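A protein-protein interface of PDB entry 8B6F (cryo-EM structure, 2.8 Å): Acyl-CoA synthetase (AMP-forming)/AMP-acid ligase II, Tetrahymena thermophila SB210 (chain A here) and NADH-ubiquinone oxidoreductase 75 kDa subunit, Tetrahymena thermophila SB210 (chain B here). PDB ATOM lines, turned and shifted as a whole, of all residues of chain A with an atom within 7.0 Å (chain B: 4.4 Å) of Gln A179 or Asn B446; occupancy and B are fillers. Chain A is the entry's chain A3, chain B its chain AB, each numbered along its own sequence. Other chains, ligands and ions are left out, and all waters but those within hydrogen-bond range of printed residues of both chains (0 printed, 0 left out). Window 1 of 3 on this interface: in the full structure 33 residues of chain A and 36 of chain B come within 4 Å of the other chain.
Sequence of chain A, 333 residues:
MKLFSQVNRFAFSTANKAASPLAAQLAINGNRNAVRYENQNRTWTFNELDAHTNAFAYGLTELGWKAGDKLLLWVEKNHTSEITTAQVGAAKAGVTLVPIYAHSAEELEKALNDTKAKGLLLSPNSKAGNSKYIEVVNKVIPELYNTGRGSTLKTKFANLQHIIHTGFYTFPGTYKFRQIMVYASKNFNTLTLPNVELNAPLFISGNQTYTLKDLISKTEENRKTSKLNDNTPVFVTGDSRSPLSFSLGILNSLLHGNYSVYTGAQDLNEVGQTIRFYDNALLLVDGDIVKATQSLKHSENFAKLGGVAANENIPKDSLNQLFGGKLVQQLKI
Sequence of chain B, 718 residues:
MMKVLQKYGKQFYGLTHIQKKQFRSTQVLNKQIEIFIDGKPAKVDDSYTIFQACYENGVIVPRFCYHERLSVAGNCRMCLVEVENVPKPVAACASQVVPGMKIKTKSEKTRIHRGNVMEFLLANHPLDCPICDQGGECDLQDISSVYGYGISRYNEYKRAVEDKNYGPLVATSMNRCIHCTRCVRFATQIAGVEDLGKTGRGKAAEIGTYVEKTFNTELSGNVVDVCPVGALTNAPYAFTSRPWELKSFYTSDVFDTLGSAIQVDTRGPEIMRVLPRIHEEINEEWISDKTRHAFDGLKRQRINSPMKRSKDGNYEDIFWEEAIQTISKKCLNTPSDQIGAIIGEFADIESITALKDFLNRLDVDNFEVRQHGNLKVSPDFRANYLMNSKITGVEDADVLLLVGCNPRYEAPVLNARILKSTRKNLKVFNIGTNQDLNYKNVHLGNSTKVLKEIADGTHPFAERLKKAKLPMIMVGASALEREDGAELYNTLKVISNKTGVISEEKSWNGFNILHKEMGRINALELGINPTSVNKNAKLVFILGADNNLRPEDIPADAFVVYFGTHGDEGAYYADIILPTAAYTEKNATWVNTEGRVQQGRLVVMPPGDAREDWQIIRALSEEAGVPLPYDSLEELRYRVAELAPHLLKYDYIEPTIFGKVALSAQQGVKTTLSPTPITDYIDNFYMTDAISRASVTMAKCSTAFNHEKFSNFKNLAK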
ATOM      1  N   TYR A  58     -21.277  13.205   1.711  1.00  0.00           N
ATOM      2  CA  TYR A  58     -21.246  14.446   2.475  1.00  0.00           C
ATOM      3  C   TYR A  58     -19.823  14.964   2.624  1.00  0.00           C
ATOM      4  O   TYR A  58     -19.582  16.173   2.531  1.00  0.00           O
ATOM      5  CB  TYR A  58     -21.882  14.236   3.849  1.00  0.00           C
ATOM      6  CG  TYR A  58     -23.390  14.323   3.844  1.00  0.00           C
ATOM      7  CD1 TYR A  58     -24.035  15.521   3.565  1.00  0.00           C
ATOM      8  CD2 TYR A  58     -24.169  13.213   4.134  1.00  0.00           C
ATOM      9  CE1 TYR A  58     -25.411  15.608   3.563  1.00  0.00           C
ATOM     10  CE2 TYR A  58     -25.547  13.288   4.136  1.00  0.00           C
ATOM     11  CZ  TYR A  58     -26.163  14.488   3.849  1.00  0.00           C
ATOM     12  OH  TYR A  58     -27.535  14.569   3.852  1.00  0.00           O
ATOM     13  N   GLY A  59     -18.864  14.068   2.855  1.00  0.00           N
ATOM     14  CA  GLY A  59     -17.478  14.499   2.929  1.00  0.00           C
ATOM     15  C   GLY A  59     -17.010  15.155   1.644  1.00  0.00           C
ATOM     16  O   GLY A  59     -16.398  16.226   1.666  1.00  0.00           O
ATOM     17  N   LEU A  60     -17.305  14.530   0.503  1.00  0.00           N
ATOM     18  CA  LEU A  60     -16.920  15.121  -0.775  1.00  0.00           C
ATOM     19  C   LEU A  60     -17.589  16.474  -0.976  1.00  0.00           C
ATOM     20  O   LEU A  60     -16.945  17.436  -1.410  1.00  0.00           O
ATOM     21  CB  LEU A  60     -17.270  14.172  -1.921  1.00  0.00           C
ATOM     22  CG  LEU A  60     -16.142  13.232  -2.355  1.00  0.00           C
ATOM     23  CD1 LEU A  60     -15.690  12.349  -1.203  1.00  0.00           C
ATOM     24  CD2 LEU A  60     -16.583  12.388  -3.539  1.00  0.00           C
ATOM     25  N   GLU A  62     -18.675  18.594   1.283  1.00  0.00           N
ATOM     26  CA  GLU A  62     -18.062  19.580   2.166  1.00  0.00           C
ATOM     27  C   GLU A  62     -16.711  20.031   1.631  1.00  0.00           C
ATOM     28  O   GLU A  62     -16.391  21.226   1.662  1.00  0.00           O
ATOM     29  CB  GLU A  62     -17.916  19.001   3.575  1.00  0.00           C
ATOM     30  CG  GLU A  62     -17.385  19.996   4.596  1.00  0.00           C
ATOM     31  CD  GLU A  62     -17.283  19.405   5.989  1.00  0.00           C
ATOM     32  OE1 GLU A  62     -17.613  18.213   6.156  1.00  0.00           O
ATOM     33  OE2 GLU A  62     -16.871  20.133   6.917  1.00  0.00           O
ATOM     34  N   LEU A  63     -15.904  19.095   1.132  1.00  0.00           N
ATOM     35  CA  LEU A  63     -14.628  19.469   0.529  1.00  0.00           C
ATOM     36  C   LEU A  63     -14.828  20.354  -0.693  1.00  0.00           C
ATOM     37  O   LEU A  63     -13.938  21.136  -1.043  1.00  0.00           O
ATOM     38  CB  LEU A  63     -13.839  18.216   0.152  1.00  0.00           C
ATOM     39  CG  LEU A  63     -13.435  17.318   1.322  1.00  0.00           C
ATOM     40  CD1 LEU A  63     -12.743  16.067   0.816  1.00  0.00           C
ATOM     41  CD2 LEU A  63     -12.546  18.053   2.306  1.00  0.00           C
ATOM     42  N   HIS A 165      -5.459   8.419   0.356  1.00  0.00           N
ATOM     43  CA  HIS A 165      -4.834   7.105   0.405  1.00  0.00           C
ATOM     44  C   HIS A 165      -5.551   6.236   1.427  1.00  0.00           C
ATOM     45  O   HIS A 165      -5.893   6.699   2.518  1.00  0.00           O
ATOM     46  CB  HIS A 165      -3.342   7.196   0.761  1.00  0.00           C
ATOM     47  CG  HIS A 165      -3.073   7.638   2.167  1.00  0.00           C
ATOM     48  ND1 HIS A 165      -3.768   8.660   2.781  1.00  0.00           N
ATOM     49  CD2 HIS A 165      -2.187   7.185   3.085  1.00  0.00           C
ATOM     50  CE1 HIS A 165      -3.317   8.819   4.011  1.00  0.00           C
ATOM     51  NE2 HIS A 165      -2.358   7.937   4.221  1.00  0.00           N
ATOM     52  N   THR A 170      -0.053   8.235   7.612  1.00  0.00           N
ATOM     53  CA  THR A 170      -0.398   9.496   6.974  1.00  0.00           C
ATOM     54  C   THR A 170       0.847  10.099   6.337  1.00  0.00           C
ATOM     55  O   THR A 170       1.956   9.966   6.859  1.00  0.00           O
ATOM     56  CB  THR A 170      -1.002  10.492   7.977  1.00  0.00           C
ATOM     57  OG1 THR A 170      -1.557  11.608   7.269  1.00  0.00           O
ATOM     58  CG2 THR A 170       0.058  11.007   8.939  1.00  0.00           C
ATOM     59  N   THR A 174      -1.692  14.513   1.759  1.00  0.00           N
ATOM     60  CA  THR A 174      -2.662  13.445   1.569  1.00  0.00           C
ATOM     61  C   THR A 174      -3.558  13.365   2.796  1.00  0.00           C
ATOM     62  O   THR A 174      -3.177  13.775   3.896  1.00  0.00           O
ATOM     63  CB  THR A 174      -1.971  12.094   1.329  1.00  0.00           C
ATOM     64  OG1 THR A 174      -0.939  12.248   0.347  1.00  0.00           O
ATOM     65  CG2 THR A 174      -2.969  11.055   0.839  1.00  0.00           C
ATOM     66  N   TYR A 175      -4.762  12.835   2.594  1.00  0.00           N
ATOM     67  CA  TYR A 175      -5.733  12.661   3.661  1.00  0.00           C
ATOM     68  C   TYR A 175      -6.268  11.237   3.621  1.00  0.00           C
ATOM     69  O   TYR A 175      -6.348  10.618   2.558  1.00  0.00           O
ATOM     70  CB  TYR A 175      -6.888  13.662   3.538  1.00  0.00           C
ATOM     71  CG  TYR A 175      -6.428  15.092   3.384  1.00  0.00           C
ATOM     72  CD1 TYR A 175      -6.014  15.831   4.484  1.00  0.00           C
ATOM     73  CD2 TYR A 175      -6.406  15.702   2.137  1.00  0.00           C
ATOM     74  CE1 TYR A 175      -5.590  17.139   4.349  1.00  0.00           C
ATOM     75  CE2 TYR A 175      -5.982  17.008   1.989  1.00  0.00           C
ATOM     76  CZ  TYR A 175      -5.577  17.721   3.098  1.00  0.00           C
ATOM     77  OH  TYR A 175      -5.156  19.023   2.957  1.00  0.00           O
ATOM     78  N   LYS A 176      -6.623  10.720   4.793  1.00  0.00           N
ATOM     79  CA  LYS A 176      -7.097   9.350   4.896  1.00  0.00           C
ATOM     80  C   LYS A 176      -8.584   9.266   4.564  1.00  0.00           C
ATOM     81  O   LYS A 176      -9.326  10.247   4.640  1.00  0.00           O
ATOM     82  CB  LYS A 176      -6.833   8.794   6.296  1.00  0.00           C
ATOM     83  CG  LYS A 176      -5.364   8.484   6.551  1.00  0.00           C
ATOM     84  CD  LYS A 176      -5.119   7.978   7.964  1.00  0.00           C
ATOM     85  CE  LYS A 176      -5.299   9.082   8.991  1.00  0.00           C
ATOM     86  NZ  LYS A 176      -4.929   8.631  10.361  1.00  0.00           N
ATOM     87  N   PHE A 177      -9.015   8.057   4.199  1.00  0.00           N
ATOM     88  CA  PHE A 177     -10.401   7.854   3.790  1.00  0.00           C
ATOM     89  C   PHE A 177     -11.362   8.190   4.923  1.00  0.00           C
ATOM     90  O   PHE A 177     -12.391   8.841   4.701  1.00  0.00           O
ATOM     91  CB  PHE A 177     -10.595   6.411   3.323  1.00  0.00           C
ATOM     92  CG  PHE A 177     -11.765   6.224   2.402  1.00  0.00           C
ATOM     93  CD1 PHE A 177     -11.606   6.359   1.032  1.00  0.00           C
ATOM     94  CD2 PHE A 177     -13.016   5.901   2.897  1.00  0.00           C
ATOM     95  CE1 PHE A 177     -12.675   6.188   0.176  1.00  0.00           C
ATOM     96  CE2 PHE A 177     -14.088   5.726   2.040  1.00  0.00           C
ATOM     97  CZ  PHE A 177     -13.916   5.868   0.681  1.00  0.00           C
ATOM     98  N   ARG A 178     -11.045   7.762   6.144  1.00  0.00           N
ATOM     99  CA  ARG A 178     -11.898   8.086   7.282  1.00  0.00           C
ATOM    100  C   ARG A 178     -11.936   9.587   7.528  1.00  0.00           C
ATOM    101  O   ARG A 178     -12.997  10.150   7.825  1.00  0.00           O
ATOM    102  CB  ARG A 178     -11.418   7.350   8.531  1.00  0.00           C
ATOM    103  CG  ARG A 178     -12.310   7.578   9.735  1.00  0.00           C
ATOM    104  CD  ARG A 178     -12.237   6.426  10.718  1.00  0.00           C
ATOM    105  NE  ARG A 178     -13.286   6.524  11.724  1.00  0.00           N
ATOM    106  CZ  ARG A 178     -13.584   5.572  12.595  1.00  0.00           C
ATOM    107  NH1 ARG A 178     -12.924   4.426  12.619  1.00  0.00           N
ATOM    108  NH2 ARG A 178     -14.568   5.775  13.466  1.00  0.00           N
ATOM    109  N   GLN A 179     -10.788  10.255   7.407  1.00  0.00           N
ATOM    110  CA  GLN A 179     -10.754  11.703   7.581  1.00  0.00           C
ATOM    111  C   GLN A 179     -11.633  12.398   6.551  1.00  0.00           C
ATOM    112  O   GLN A 179     -12.292  13.398   6.857  1.00  0.00           O
ATOM    113  CB  GLN A 179      -9.315  12.210   7.494  1.00  0.00           C
ATOM    114  CG  GLN A 179      -8.406  11.653   8.579  1.00  0.00           C
ATOM    115  CD  GLN A 179      -6.986  12.165   8.466  1.00  0.00           C
ATOM    116  OE1 GLN A 179      -6.597  12.738   7.450  1.00  0.00           O
ATOM    117  NE2 GLN A 179      -6.201  11.964   9.519  1.00  0.00           N
ATOM    118  N   ILE A 180     -11.651  11.889   5.318  1.00  0.00           N
ATOM    119  CA  ILE A 180     -12.518  12.459   4.293  1.00  0.00           C
ATOM    120  C   ILE A 180     -13.984  12.217   4.640  1.00  0.00           C
ATOM    121  O   ILE A 180     -14.835  13.089   4.429  1.00  0.00           O
ATOM    122  CB  ILE A 180     -12.153  11.877   2.915  1.00  0.00           C
ATOM    123  CG1 ILE A 180     -10.716  12.262   2.537  1.00  0.00           C
ATOM    124  CG2 ILE A 180     -13.148  12.337   1.846  1.00  0.00           C
ATOM    125  CD1 ILE A 180     -10.515  13.720   2.183  1.00  0.00           C
ATOM    126  N   MET A 181     -14.304  11.039   5.172  1.00  0.00           N
ATOM    127  CA  MET A 181     -15.686  10.719   5.507  1.00  0.00           C
ATOM    128  C   MET A 181     -16.254  11.708   6.516  1.00  0.00           C
ATOM    129  O   MET A 181     -15.568  12.144   7.443  1.00  0.00           O
ATOM    130  CB  MET A 181     -15.798   9.303   6.069  1.00  0.00           C
ATOM    131  CG  MET A 181     -16.091   8.248   5.026  1.00  0.00           C
ATOM    132  SD  MET A 181     -16.565   6.686   5.784  1.00  0.00           S
ATOM    133  CE  MET A 181     -16.983   5.744   4.328  1.00  0.00           C
ATOM    134  N   VAL A 182     -17.527  12.059   6.328  1.00  0.00           N
ATOM    135  CA  VAL A 182     -18.237  12.978   7.209  1.00  0.00           C
ATOM    136  C   VAL A 182     -19.645  12.429   7.412  1.00  0.00           C
ATOM    137  O   VAL A 182     -20.455  12.435   6.480  1.00  0.00           O
ATOM    138  CB  VAL A 182     -18.296  14.403   6.642  1.00  0.00           C
ATOM    139  CG1 VAL A 182     -19.112  15.310   7.552  1.00  0.00           C
ATOM    140  CG2 VAL A 182     -16.894  14.952   6.448  1.00  0.00           C
ATOM    141  N   GLY B 432     -14.074  17.360  12.820  1.00  0.00           N
ATOM    142  CA  GLY B 432     -12.821  16.788  12.382  1.00  0.00           C
ATOM    143  C   GLY B 432     -13.042  15.361  11.901  1.00  0.00           C
ATOM    144  O   GLY B 432     -14.034  15.073  11.229  1.00  0.00           O
ATOM    145  N   THR B 433     -12.106  14.489  12.253  1.00  0.00           N
ATOM    146  CA  THR B 433     -12.233  13.079  11.927  1.00  0.00           C
ATOM    147  C   THR B 433     -13.253  12.418  12.846  1.00  0.00           C
ATOM    148  O   THR B 433     -13.486  12.862  13.974  1.00  0.00           O
ATOM    149  CB  THR B 433     -10.881  12.374  12.051  1.00  0.00           C
ATOM    150  OG1 THR B 433      -9.888  13.109  11.326  1.00  0.00           O
ATOM    151  CG2 THR B 433     -10.953  10.959  11.496  1.00  0.00           C
ATOM    152  N   HIS B 443     -21.171  14.172  14.744  1.00  0.00           N
ATOM    153  CA  HIS B 443     -20.094  14.596  13.851  1.00  0.00           C
ATOM    154  C   HIS B 443     -20.613  15.731  12.976  1.00  0.00           C
ATOM    155  O   HIS B 443     -21.351  15.501  12.016  1.00  0.00           O
ATOM    156  CB  HIS B 443     -19.596  13.425  13.015  1.00  0.00           C
ATOM    157  CG  HIS B 443     -18.348  13.722  12.244  1.00  0.00           C
ATOM    158  ND1 HIS B 443     -17.987  13.019  11.115  1.00  0.00           N
ATOM    159  CD2 HIS B 443     -17.375  14.640  12.442  1.00  0.00           C
ATOM    160  CE1 HIS B 443     -16.847  13.495  10.649  1.00  0.00           C
ATOM    161  NE2 HIS B 443     -16.453  14.479  11.436  1.00  0.00           N
ATOM    162  N   GLY B 445     -18.697  17.903  11.144  1.00  0.00           N
ATOM    163  CA  GLY B 445     -17.958  17.982   9.901  1.00  0.00           C
ATOM    164  C   GLY B 445     -16.478  17.785  10.144  1.00  0.00           C
ATOM    165  O   GLY B 445     -16.038  17.497  11.261  1.00  0.00           O
ATOM    166  N   ASN B 446     -15.712  17.945   9.063  1.00  0.00           N
ATOM    167  CA  ASN B 446     -14.263  17.820   9.121  1.00  0.00           C
ATOM    168  C   ASN B 446     -13.518  19.012   8.541  1.00  0.00           C
ATOM    169  O   ASN B 446     -12.306  19.118   8.761  1.00  0.00           O
ATOM    170  CB  ASN B 446     -13.800  16.551   8.389  1.00  0.00           C
ATOM    171  CG  ASN B 446     -14.178  16.550   6.921  1.00  0.00           C
ATOM    172  OD1 ASN B 446     -14.721  17.527   6.405  1.00  0.00           O
ATOM    173  ND2 ASN B 446     -13.882  15.452   6.237  1.00  0.00           N
ATOM    174  N   SER B 447     -14.186  19.902   7.816  1.00  0.00           N
ATOM    175  CA  SER B 447     -13.548  21.050   7.197  1.00  0.00           C
ATOM    176  C   SER B 447     -13.717  22.284   8.077  1.00  0.00           C
ATOM    177  O   SER B 447     -14.355  22.251   9.131  1.00  0.00           O
ATOM    178  CB  SER B 447     -14.130  21.289   5.802  1.00  0.00           C
ATOM    179  OG  SER B 447     -13.569  22.445   5.203  1.00  0.00           O
ATOM    180  N   THR B 676      -9.782  22.765   4.004  1.00  0.00           N
ATOM    181  CA  THR B 676      -9.088  21.490   4.094  1.00  0.00           C
ATOM    182  C   THR B 676      -9.563  20.745   5.332  1.00  0.00           C
ATOM    183  O   THR B 676     -10.018  21.372   6.295  1.00  0.00           O
ATOM    184  CB  THR B 676      -7.565  21.692   4.154  1.00  0.00           C
ATOM    185  OG1 THR B 676      -6.906  20.424   4.256  1.00  0.00           O
ATOM    186  CG2 THR B 676      -7.188  22.560   5.341  1.00  0.00           C
ATOM    187  N   PRO B 677      -9.476  19.414   5.337  1.00  0.00           N
ATOM    188  CA  PRO B 677      -9.923  18.657   6.511  1.00  0.00           C
ATOM    189  C   PRO B 677      -9.071  18.941   7.739  1.00  0.00           C
ATOM    190  O   PRO B 677      -7.886  19.267   7.643  1.00  0.00           O
ATOM    191  CB  PRO B 677      -9.779  17.193   6.075  1.00  0.00           C
ATOM    192  CG  PRO B 677      -9.712  17.225   4.600  1.00  0.00           C
ATOM    193  CD  PRO B 677      -9.076  18.523   4.234  1.00  0.00           C
ATOM    194  N   ILE B 678      -9.697  18.809   8.905  1.00  0.00           N
ATOM    195  CA  ILE B 678      -9.005  18.849  10.188  1.00  0.00           C
ATOM    196  C   ILE B 678      -8.710  17.412  10.595  1.00  0.00           C
ATOM    197  O   ILE B 678      -9.624  16.582  10.675  1.00  0.00           O
ATOM    198  CB  ILE B 678      -9.844  19.564  11.259  1.00  0.00           C
ATOM    199  CG1 ILE B 678     -10.318  20.932  10.755  1.00  0.00           C
ATOM    200  CG2 ILE B 678      -9.045  19.718  12.546  1.00  0.00           C
ATOM    201  CD1 ILE B 678      -9.201  21.879  10.365  1.00  0.00           C
ATOM    202  N   THR B 679      -7.442  17.113  10.853  1.00  0.00           N
ATOM    203  CA  THR B 679      -6.982  15.750  11.082  1.00  0.00           C
ATOM    204  C   THR B 679      -6.394  15.621  12.484  1.00  0.00           C
ATOM    205  O   THR B 679      -6.323  16.585  13.248  1.00  0.00           O
ATOM    206  CB  THR B 679      -5.950  15.343  10.026  1.00  0.00           C
ATOM    207  OG1 THR B 679      -4.800  16.193  10.121  1.00  0.00           O
ATOM    208  CG2 THR B 679      -6.542  15.455   8.629  1.00  0.00           C
ATOM    209  N   ASP B 680      -5.973  14.400  12.813  1.00  0.00           N
ATOM    210  CA  ASP B 680      -5.332  14.087  14.082  1.00  0.00           C
ATOM    211  C   ASP B 680      -3.937  13.543  13.813  1.00  0.00           C
ATOM    212  O   ASP B 680      -3.737  12.754  12.883  1.00  0.00           O
ATOM    213  CB  ASP B 680      -6.148  13.066  14.878  1.00  0.00           C
ATOM    214  CG  ASP B 680      -7.584  13.505  15.085  1.00  0.00           C
ATOM    215  OD1 ASP B 680      -7.835  14.728  15.100  1.00  0.00           O
ATOM    216  OD2 ASP B 680      -8.461  12.629  15.230  1.00  0.00           O
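OE1 of Glu A62 lies close to OD1 of Asn B446.
ND2 of Asn B446 is in hydrogen-bond range of O of Gln A179 (2.7 Å).
The side-chain amide nitrogen of Asn B446 sits at hydrogen-bond distance from the backbone carbonyl oxygen of Ile A180 (3.1 Å).
The backbone NH (N) of Ser B447 lies within hydrogen-bond range of the side-chain carboxylate (OE2) of Glu A62 (2.8 Å).
OG1 of Thr B676 is in hydrogen-bond range of OH of Tyr A175, 2.6 Å away.
The backbone carbonyl oxygen (O) of Gly B432 lies within hydrogen-bond range of a ring nitrogen (NE2) of His B443 (2.5 Å).
The backbone NH (N) of Gly B432 sits at hydrogen-bond distance from the backbone carbonyl oxygen (O) of Gly B445, 2.5 Å away.
NE2 of His B443 lies within hydrogen-bond range of O of Gly B445 (3.1 Å).
The backbone NH (N) of Ile B678 is in hydrogen-bond range of the backbone carbonyl oxygen (O) of Asn B446, at 2.6 Å.
The backbone NH (N) of His A165 sits at hydrogen-bond distance from the backbone carbonyl oxygen (O) of Tyr A175 (3.2 Å).
N of Lys A176 lies within hydrogen-bond range of OE1 of Gln A179.
OE1 of Glu A62 touches CA of Gly B445, at 3.8 Å.
CD2 of Leu A63 touches CG of Pro B677, 3.7 Å away.
Tyr A175 touches Pro B677 (CE1 to CD, 3.8 Å).
Thr B433 touches Gln A179 (OG1 to CG, 3.4 Å).
CG2 of Thr B679 touches OE1 of Gln A179 (3.0 Å).
Met A181 touches His B443.
ND2 of Asn B446 touches O of Met A181 (3.9 Å).
His B443 touches Val A182.
Val A182 touches Gly B445.
Asn B446 touches Val A182.
Phe A177 touches none of the printed residues of chain B.
Of the printed residues of chain B, Ile A180 touches Asn B446 (3.1 Å).
Asn B446 touches just these residues of chain A: Glu A62 (3.0 Å), Gln A179 (2.7 Å), Ile A180 (3.1 Å), Met A181 (3.9 Å) and Val A182 (3.1 Å).
Printed residues of chain A within 4 Å of Ser B447: Glu A62 (2.8 Å).
Of the printed residues of chain A, Pro B677 touches Leu A63 (3.7 Å) and Tyr A175 (3.8 Å).
Ile B678 touches none of the printed residues of chain A.
Of the printed residues of chain A, Thr B679 touches Gln A179 (3.0 Å).
The nearest printed residue of chain A that does not touch His B443 is Arg A178 (5.8 Å).
Hydrophobic or aromatic side chains of chain B that line the printed part of chain A: His B443 and Pro B677.
Of the 16 printed residues of chain A, 7 touch a printed residue of chain B.
Hydrophobic or aromatic side chains of chain A within 4 Å of the printed part of chain B: Leu A63, Tyr A175 and Val A182.
Along chain A the printed residues that touch a printed residue of chain B span positions 62 to 182.
Among the printed residues, 15 pairs touch across the chains.
Among the printed residues, no Asp or Glu carboxylate lies within 4 Å of a Lys or Arg side-chain nitrogen of the other chain.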
